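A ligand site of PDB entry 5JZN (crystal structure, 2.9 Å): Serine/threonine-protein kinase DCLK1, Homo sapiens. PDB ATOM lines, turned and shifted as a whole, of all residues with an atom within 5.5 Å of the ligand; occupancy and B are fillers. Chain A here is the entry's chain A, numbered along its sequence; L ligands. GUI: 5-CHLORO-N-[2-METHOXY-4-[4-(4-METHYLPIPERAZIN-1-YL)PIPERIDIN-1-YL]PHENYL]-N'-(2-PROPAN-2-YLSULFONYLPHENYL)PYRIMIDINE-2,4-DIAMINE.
NZ of Lys 50 lies within salt-bridge range of OD1 of Asp 164 (3.8 Å). The backbone carbonyl oxygen of Val 35 sits at hydrogen-bond distance from the backbone NH of Ile 27, at 2.9 Å. The backbone NH of Gly 163 lies within hydrogen-bond range of the backbone carbonyl oxygen of Asn 147 (3.0 Å). N of Asp 106 sits at hydrogen-bond distance from OD1 of Asp 103. The backbone NH (N) of Val 35 lies within hydrogen-bond range of the backbone carbonyl oxygen (O) of Gly 28 (3.2 Å). The side-chain amino group of Lys 100 is in salt-bridge range of the side-chain carboxylate of Glu 37. The side-chain carboxylate of Glu 37 lies within salt-bridge range of the guanidinium group of Arg 25 (3.97 Å). O of Met 96 lies within hydrogen-bond range of N of Ala 48.
The backbone NH (N) of Val 99 sits at hydrogen-bond distance from a nitrogen (N5) of the ligand, 3.0 Å away. A nitrogen (N7) of the ligand lies within hydrogen-bond range of the backbone carbonyl oxygen of Val 99, at 2.7 Å. The side-chain amino group of Lys 50 lies within hydrogen-bond range of an oxygen (O41) of the ligand (3.2 Å). OD2 of Asp 106 lies within salt-bridge range of N22 of the ligand.
Ile 27 touches the ligand. Gly 28 touches the ligand. CG2 of Val 35 touches C30 of the ligand, 3.7 Å away. Glu 37 touches the ligand (OE2 to C15, 3.8 Å). Ala 48 touches the ligand. Glu 97 touches the ligand. CA of Leu 98 touches N5 of the ligand (3.8 Å). Lys 100 touches the ligand (O to O14, 3.7 Å). Gly 102 touches the ligand. Glu 146 touches the ligand (O to C39, 3.4 Å). Asn 147 touches the ligand. CD1 of Leu 149 touches C6 of the ligand, at 3.4 Å. Asp 164 touches the ligand (OD1 to O40, 3.9 Å). 16 residues have an atom within 4 Å of the ligand: Ile 27, Gly 28, Val 35, Glu 37, Ala 48, Lys 50, Glu 97, Leu 98, Val 99, Lys 100, Gly 102, Asp 106, Glu 146, Asn 147, Leu 149 and Asp 164.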
ATOM      1  N   ARG A  25     -23.335   8.343  20.429  1.00  0.00           N
ATOM      2  CA  ARG A  25     -23.199   7.532  19.239  1.00  0.00           C
ATOM      3  C   ARG A  25     -24.403   6.606  19.004  1.00  0.00           C
ATOM      4  O   ARG A  25     -25.114   6.204  19.932  1.00  0.00           O
ATOM      5  CB  ARG A  25     -21.927   6.664  19.462  1.00  0.00           C
ATOM      6  CG  ARG A  25     -22.169   5.164  19.292  1.00  0.00           C
ATOM      7  CD  ARG A  25     -20.986   4.213  19.569  1.00  0.00           C
ATOM      8  NE  ARG A  25     -21.540   2.867  19.793  1.00  0.00           N
ATOM      9  CZ  ARG A  25     -20.954   1.861  20.441  1.00  0.00           C
ATOM     10  NH1 ARG A  25     -19.772   2.019  20.993  1.00  0.00           N
ATOM     11  NH2 ARG A  25     -21.583   0.679  20.555  1.00  0.00           N
ATOM     12  N   ILE A  27     -26.061   3.171  18.325  1.00  0.00           N
ATOM     13  CA  ILE A  27     -25.661   1.804  18.678  1.00  0.00           C
ATOM     14  C   ILE A  27     -26.448   0.797  17.860  1.00  0.00           C
ATOM     15  O   ILE A  27     -26.122  -0.381  17.814  1.00  0.00           O
ATOM     16  CB  ILE A  27     -25.776   1.490  20.181  1.00  0.00           C
ATOM     17  CG1 ILE A  27     -27.125   1.901  20.731  1.00  0.00           C
ATOM     18  CG2 ILE A  27     -24.681   2.208  20.943  1.00  0.00           C
ATOM     19  CD1 ILE A  27     -27.375   1.329  22.127  1.00  0.00           C
ATOM     20  N   GLY A  28     -27.481   1.270  17.162  1.00  0.00           N
ATOM     21  CA  GLY A  28     -28.273   0.408  16.314  1.00  0.00           C
ATOM     22  C   GLY A  28     -29.161   1.268  15.438  1.00  0.00           C
ATOM     23  O   GLY A  28     -29.460   2.411  15.766  1.00  0.00           O
ATOM     24  N   ASP A  29     -29.629   0.684  14.345  1.00  0.00           N
ATOM     25  CA  ASP A  29     -30.486   1.368  13.384  1.00  0.00           C
ATOM     26  C   ASP A  29     -31.413   0.377  12.713  1.00  0.00           C
ATOM     27  O   ASP A  29     -31.019  -0.747  12.416  1.00  0.00           O
ATOM     28  CB  ASP A  29     -29.662   2.121  12.336  1.00  0.00           C
ATOM     29  N   ALA A  33     -36.932   2.495  14.186  1.00  0.00           N
ATOM     30  CA  ALA A  33     -36.322   3.182  15.326  1.00  0.00           C
ATOM     31  C   ALA A  33     -34.816   3.399  15.129  1.00  0.00           C
ATOM     32  O   ALA A  33     -34.160   2.662  14.397  1.00  0.00           O
ATOM     33  CB  ALA A  33     -36.577   2.400  16.616  1.00  0.00           C
ATOM     34  N   VAL A  35     -31.466   3.837  17.762  1.00  0.00           N
ATOM     35  CA  VAL A  35     -31.128   3.820  19.189  1.00  0.00           C
ATOM     36  C   VAL A  35     -29.724   4.387  19.414  1.00  0.00           C
ATOM     37  O   VAL A  35     -28.761   3.974  18.763  1.00  0.00           O
ATOM     38  CB  VAL A  35     -31.233   2.421  19.792  1.00  0.00           C
ATOM     39  CG1 VAL A  35     -30.940   2.466  21.284  1.00  0.00           C
ATOM     40  CG2 VAL A  35     -32.622   1.879  19.553  1.00  0.00           C
ATOM     41  N   GLU A  37     -26.622   5.880  22.270  1.00  0.00           N
ATOM     42  CA  GLU A  37     -26.080   5.954  23.622  1.00  0.00           C
ATOM     43  C   GLU A  37     -26.299   7.391  24.046  1.00  0.00           C
ATOM     44  O   GLU A  37     -26.223   8.302  23.230  1.00  0.00           O
ATOM     45  CB  GLU A  37     -24.597   5.576  23.626  1.00  0.00           C
ATOM     46  CG  GLU A  37     -24.310   4.105  23.987  1.00  0.00           C
ATOM     47  CD  GLU A  37     -22.825   3.723  23.879  1.00  0.00           C
ATOM     48  OE1 GLU A  37     -22.042   4.542  23.355  1.00  0.00           O
ATOM     49  OE2 GLU A  37     -22.472   2.594  24.294  1.00  0.00           O
ATOM     50  N   ALA A  48     -29.839   4.511  27.180  1.00  0.00           N
ATOM     51  CA  ALA A  48     -30.096   4.412  25.746  1.00  0.00           C
ATOM     52  C   ALA A  48     -31.234   5.359  25.369  1.00  0.00           C
ATOM     53  O   ALA A  48     -32.204   5.483  26.104  1.00  0.00           O
ATOM     54  CB  ALA A  48     -30.448   2.987  25.357  1.00  0.00           C
ATOM     55  N   LYS A  50     -33.961   5.687  22.604  1.00  0.00           N
ATOM     56  CA  LYS A  50     -34.619   5.046  21.479  1.00  0.00           C
ATOM     57  C   LYS A  50     -35.527   6.050  20.800  1.00  0.00           C
ATOM     58  O   LYS A  50     -36.428   6.621  21.427  1.00  0.00           O
ATOM     59  CB  LYS A  50     -35.343   3.814  22.002  1.00  0.00           C
ATOM     60  CG  LYS A  50     -36.145   2.982  21.042  1.00  0.00           C
ATOM     61  CD  LYS A  50     -36.395   1.675  21.818  1.00  0.00           C
ATOM     62  CE  LYS A  50     -37.476   0.763  21.283  1.00  0.00           C
ATOM     63  NZ  LYS A  50     -37.458  -0.485  22.106  1.00  0.00           N
ATOM     64  N   VAL A  80     -36.105  -4.449  30.297  1.00  0.00           N
ATOM     65  CA  VAL A  80     -35.385  -3.190  30.150  1.00  0.00           C
ATOM     66  C   VAL A  80     -36.247  -2.102  30.742  1.00  0.00           C
ATOM     67  O   VAL A  80     -37.414  -1.949  30.368  1.00  0.00           O
ATOM     68  CB  VAL A  80     -35.073  -2.864  28.670  1.00  0.00           C
ATOM     69  CG1 VAL A  80     -34.282  -1.567  28.568  1.00  0.00           C
ATOM     70  CG2 VAL A  80     -34.299  -4.008  28.027  1.00  0.00           C
ATOM     71  N   MET A  96     -33.976   4.748  28.012  1.00  0.00           N
ATOM     72  CA  MET A  96     -34.077   3.448  28.657  1.00  0.00           C
ATOM     73  C   MET A  96     -32.740   3.011  29.214  1.00  0.00           C
ATOM     74  O   MET A  96     -31.703   3.500  28.768  1.00  0.00           O
ATOM     75  CB  MET A  96     -34.612   2.426  27.671  1.00  0.00           C
ATOM     76  CG  MET A  96     -35.986   2.807  27.176  1.00  0.00           C
ATOM     77  SD  MET A  96     -36.805   1.526  26.262  1.00  0.00           S
ATOM     78  CE  MET A  96     -37.215   0.428  27.614  1.00  0.00           C
ATOM     79  N   GLU A  97     -32.746   2.102  30.190  1.00  0.00           N
ATOM     80  CA  GLU A  97     -31.483   1.577  30.716  1.00  0.00           C
ATOM     81  C   GLU A  97     -30.663   0.967  29.607  1.00  0.00           C
ATOM     82  O   GLU A  97     -31.193   0.301  28.726  1.00  0.00           O
ATOM     83  CB  GLU A  97     -31.612   0.553  31.847  1.00  0.00           C
ATOM     84  CG  GLU A  97     -31.990  -0.837  31.429  1.00  0.00           C
ATOM     85  CD  GLU A  97     -32.060  -1.788  32.604  1.00  0.00           C
ATOM     86  OE1 GLU A  97     -30.971  -2.063  33.164  1.00  0.00           O
ATOM     87  OE2 GLU A  97     -33.165  -2.239  32.957  1.00  0.00           O
ATOM     88  N   LEU A  98     -29.381   1.279  29.608  1.00  0.00           N
ATOM     89  CA  LEU A  98     -28.486   0.757  28.611  1.00  0.00           C
ATOM     90  C   LEU A  98     -27.959  -0.593  29.122  1.00  0.00           C
ATOM     91  O   LEU A  98     -27.530  -0.721  30.276  1.00  0.00           O
ATOM     92  CB  LEU A  98     -27.336   1.732  28.374  1.00  0.00           C
ATOM     93  CG  LEU A  98     -26.202   1.333  27.456  1.00  0.00           C
ATOM     94  CD1 LEU A  98     -26.712   1.230  26.029  1.00  0.00           C
ATOM     95  CD2 LEU A  98     -25.073   2.317  27.579  1.00  0.00           C
ATOM     96  N   VAL A  99     -28.018  -1.604  28.249  1.00  0.00           N
ATOM     97  CA  VAL A  99     -27.499  -2.928  28.546  1.00  0.00           C
ATOM     98  C   VAL A  99     -26.323  -3.149  27.637  1.00  0.00           C
ATOM     99  O   VAL A  99     -26.479  -3.402  26.440  1.00  0.00           O
ATOM    100  CB  VAL A  99     -28.563  -4.035  28.328  1.00  0.00           C
ATOM    101  CG1 VAL A  99     -28.014  -5.379  28.773  1.00  0.00           C
ATOM    102  CG2 VAL A  99     -29.840  -3.711  29.085  1.00  0.00           C
ATOM    103  N   LYS A 100     -25.137  -3.039  28.232  1.00  0.00           N
ATOM    104  CA  LYS A 100     -23.861  -3.057  27.504  1.00  0.00           C
ATOM    105  C   LYS A 100     -23.481  -4.337  26.762  1.00  0.00           C
ATOM    106  O   LYS A 100     -22.754  -4.280  25.774  1.00  0.00           O
ATOM    107  CB  LYS A 100     -22.732  -2.698  28.469  1.00  0.00           C
ATOM    108  CG  LYS A 100     -22.759  -1.245  28.938  1.00  0.00           C
ATOM    109  CD  LYS A 100     -22.015  -0.383  27.918  1.00  0.00           C
ATOM    110  CE  LYS A 100     -21.507   0.928  28.490  1.00  0.00           C
ATOM    111  NZ  LYS A 100     -20.472   1.528  27.588  1.00  0.00           N
ATOM    112  N   GLY A 101     -24.002  -5.477  27.200  1.00  0.00           N
ATOM    113  CA  GLY A 101     -23.653  -6.745  26.565  1.00  0.00           C
ATOM    114  C   GLY A 101     -24.275  -6.977  25.199  1.00  0.00           C
ATOM    115  O   GLY A 101     -24.057  -8.028  24.603  1.00  0.00           O
ATOM    116  N   GLY A 102     -25.067  -6.020  24.726  1.00  0.00           N
ATOM    117  CA  GLY A 102     -25.715  -6.131  23.438  1.00  0.00           C
ATOM    118  C   GLY A 102     -26.903  -7.080  23.467  1.00  0.00           C
ATOM    119  O   GLY A 102     -27.422  -7.412  24.538  1.00  0.00           O
ATOM    120  N   ASP A 103     -27.326  -7.540  22.295  1.00  0.00           N
ATOM    121  CA  ASP A 103     -28.506  -8.409  22.234  1.00  0.00           C
ATOM    122  C   ASP A 103     -28.127  -9.876  21.996  1.00  0.00           C
ATOM    123  O   ASP A 103     -26.998 -10.205  21.625  1.00  0.00           O
ATOM    124  CB  ASP A 103     -29.517  -7.936  21.165  1.00  0.00           C
ATOM    125  CG  ASP A 103     -29.001  -8.065  19.741  1.00  0.00           C
ATOM    126  OD1 ASP A 103     -27.826  -8.447  19.548  1.00  0.00           O
ATOM    127  OD2 ASP A 103     -29.789  -7.780  18.817  1.00  0.00           O
ATOM    128  N   ASP A 106     -26.727 -11.409  18.327  1.00  0.00           N
ATOM    129  CA  ASP A 106     -25.286 -11.334  18.111  1.00  0.00           C
ATOM    130  C   ASP A 106     -24.521 -12.328  18.990  1.00  0.00           C
ATOM    131  O   ASP A 106     -23.513 -12.902  18.567  1.00  0.00           O
ATOM    132  CB  ASP A 106     -24.808  -9.925  18.397  1.00  0.00           C
ATOM    133  CG  ASP A 106     -25.245  -8.937  17.345  1.00  0.00           C
ATOM    134  OD1 ASP A 106     -25.435  -9.364  16.188  1.00  0.00           O
ATOM    135  OD2 ASP A 106     -25.447  -7.756  17.683  1.00  0.00           O
ATOM    136  N   GLU A 146     -33.320 -11.204  19.031  1.00  0.00           N
ATOM    137  CA  GLU A 146     -33.011  -9.830  18.677  1.00  0.00           C
ATOM    138  C   GLU A 146     -33.666  -8.806  19.612  1.00  0.00           C
ATOM    139  O   GLU A 146     -33.193  -7.678  19.725  1.00  0.00           O
ATOM    140  CB  GLU A 146     -33.461  -9.639  17.228  1.00  0.00           C
ATOM    141  CG  GLU A 146     -33.571  -8.234  16.716  1.00  0.00           C
ATOM    142  CD  GLU A 146     -34.304  -8.213  15.383  1.00  0.00           C
ATOM    143  OE1 GLU A 146     -34.745  -9.305  14.955  1.00  0.00           O
ATOM    144  OE2 GLU A 146     -34.406  -7.125  14.771  1.00  0.00           O
ATOM    145  N   ASN A 147     -34.710  -9.218  20.329  1.00  0.00           N
ATOM    146  CA  ASN A 147     -35.395  -8.351  21.291  1.00  0.00           C
ATOM    147  C   ASN A 147     -34.976  -8.704  22.708  1.00  0.00           C
ATOM    148  O   ASN A 147     -35.597  -8.270  23.670  1.00  0.00           O
ATOM    149  CB  ASN A 147     -36.914  -8.427  21.164  1.00  0.00           C
ATOM    150  CG  ASN A 147     -37.408  -7.787  19.873  1.00  0.00           C
ATOM    151  OD1 ASN A 147     -36.743  -6.935  19.277  1.00  0.00           O
ATOM    152  ND2 ASN A 147     -38.592  -8.201  19.433  1.00  0.00           N
ATOM    153  N   LEU A 149     -31.766  -8.590  25.452  1.00  0.00           N
ATOM    154  CA  LEU A 149     -30.446  -8.005  25.711  1.00  0.00           C
ATOM    155  C   LEU A 149     -29.654  -8.731  26.790  1.00  0.00           C
ATOM    156  O   LEU A 149     -30.227  -9.227  27.760  1.00  0.00           O
ATOM    157  CB  LEU A 149     -30.617  -6.524  26.093  1.00  0.00           C
ATOM    158  CG  LEU A 149     -31.436  -5.664  25.122  1.00  0.00           C
ATOM    159  CD1 LEU A 149     -31.515  -4.239  25.582  1.00  0.00           C
ATOM    160  CD2 LEU A 149     -30.813  -5.710  23.753  1.00  0.00           C
ATOM    161  N   GLY A 163     -36.667  -6.455  25.797  1.00  0.00           N
ATOM    162  CA  GLY A 163     -37.006  -5.100  25.393  1.00  0.00           C
ATOM    163  C   GLY A 163     -38.025  -5.027  24.274  1.00  0.00           C
ATOM    164  O   GLY A 163     -38.707  -6.007  23.975  1.00  0.00           O
ATOM    165  N   ASP A 164     -38.147  -3.852  23.648  1.00  0.00           N
ATOM    166  CA  ASP A 164     -39.025  -3.635  22.492  1.00  0.00           C
ATOM    167  C   ASP A 164     -40.451  -4.161  22.635  1.00  0.00           C
ATOM    168  O   ASP A 164     -40.770  -5.258  22.185  1.00  0.00           O
ATOM    169  CB  ASP A 164     -38.406  -4.221  21.215  1.00  0.00           C
ATOM    170  CG  ASP A 164     -39.134  -3.754  19.960  1.00  0.00           C
ATOM    171  OD1 ASP A 164     -38.648  -2.798  19.308  1.00  0.00           O
ATOM    172  OD2 ASP A 164     -40.216  -4.294  19.653  1.00  0.00           O
HETATM  173  C1  GUI L   1     -31.578  -0.745  24.693  1.00  0.00           C
HETATM  174  C2  GUI L   1     -31.066  -1.131  23.370  1.00  0.00           C
HETATM  175  N3  GUI L   1     -29.821  -1.640  23.316  1.00  0.00           N
HETATM  176  C4  GUI L   1     -29.059  -1.791  24.419  1.00  0.00           C
HETATM  177  N5  GUI L   1     -29.529  -1.419  25.633  1.00  0.00           N
HETATM  178  C6  GUI L   1     -30.755  -0.902  25.794  1.00  0.00           C
HETATM  179  N7  GUI L   1     -27.797  -2.298  24.331  1.00  0.00           N
HETATM  180  C8  GUI L   1     -27.177  -2.694  23.173  1.00  0.00           C
HETATM  181  C9  GUI L   1     -27.829  -3.317  22.117  1.00  0.00           C
HETATM  182  C10 GUI L   1     -27.126  -3.691  20.972  1.00  0.00           C
HETATM  183  C11 GUI L   1     -25.760  -3.482  20.832  1.00  0.00           C
HETATM  184  C12 GUI L   1     -25.054  -2.884  21.880  1.00  0.00           C
HETATM  185  C13 GUI L   1     -25.714  -2.479  23.035  1.00  0.00           C
HETATM  186  O14 GUI L   1     -25.033  -1.887  24.067  1.00  0.00           O
HETATM  187  C15 GUI L   1     -24.150  -0.793  23.789  1.00  0.00           C
HETATM  188  N16 GUI L   1     -25.113  -3.918  19.652  1.00  0.00           N
HETATM  189  C17 GUI L   1     -25.848  -3.506  18.443  1.00  0.00           C
HETATM  190  C18 GUI L   1     -25.274  -4.249  17.237  1.00  0.00           C
HETATM  191  C19 GUI L   1     -23.777  -4.014  17.081  1.00  0.00           C
HETATM  192  C20 GUI L   1     -23.049  -4.200  18.417  1.00  0.00           C
HETATM  193  C21 GUI L   1     -23.724  -3.438  19.559  1.00  0.00           C
HETATM  194  N22 GUI L   1     -23.194  -4.997  16.147  1.00  0.00           N
HETATM  195  C23 GUI L   1     -21.809  -4.617  15.827  1.00  0.00           C
HETATM  196  C24 GUI L   1     -21.188  -5.769  15.041  1.00  0.00           C
HETATM  197  N25 GUI L   1     -21.955  -6.039  13.818  1.00  0.00           N
HETATM  198  C26 GUI L   1     -23.379  -6.277  14.103  1.00  0.00           C
HETATM  199  C27 GUI L   1     -23.974  -5.110  14.894  1.00  0.00           C
HETATM  200  C28 GUI L   1     -21.387  -7.232  13.167  1.00  0.00           C
HETATM  201  N29 GUI L   1     -31.845  -0.997  22.262  1.00  0.00           N
HETATM  202  C30 GUI L   1     -31.545  -1.332  20.976  1.00  0.00           C
HETATM  203  C31 GUI L   1     -32.617  -1.815  20.060  1.00  0.00           C
HETATM  204  C32 GUI L   1     -32.267  -2.145  18.754  1.00  0.00           C
HETATM  205  C33 GUI L   1     -30.954  -2.045  18.295  1.00  0.00           C
HETATM  206  C34 GUI L   1     -29.956  -1.602  19.146  1.00  0.00           C
HETATM  207  C35 GUI L   1     -30.234  -1.248  20.468  1.00  0.00           C
HETATM  208  S36 GUI L   1     -34.139  -1.951  20.530  1.00  0.00           S
HETATM  209  C37 GUI L   1     -34.527  -3.505  21.034  1.00  0.00           C
HETATM  210  C38 GUI L   1     -33.668  -3.976  22.203  1.00  0.00           C
HETATM  211  C39 GUI L   1     -34.451  -4.504  19.880  1.00  0.00           C
HETATM  212  O40 GUI L   1     -34.987  -1.580  19.417  1.00  0.00           O
HETATM  213  O41 GUI L   1     -34.397  -1.076  21.636  1.00  0.00           O
HETATM  214 CL   GUI L   1     -33.231  -0.053  24.830  1.00  0.00          CL
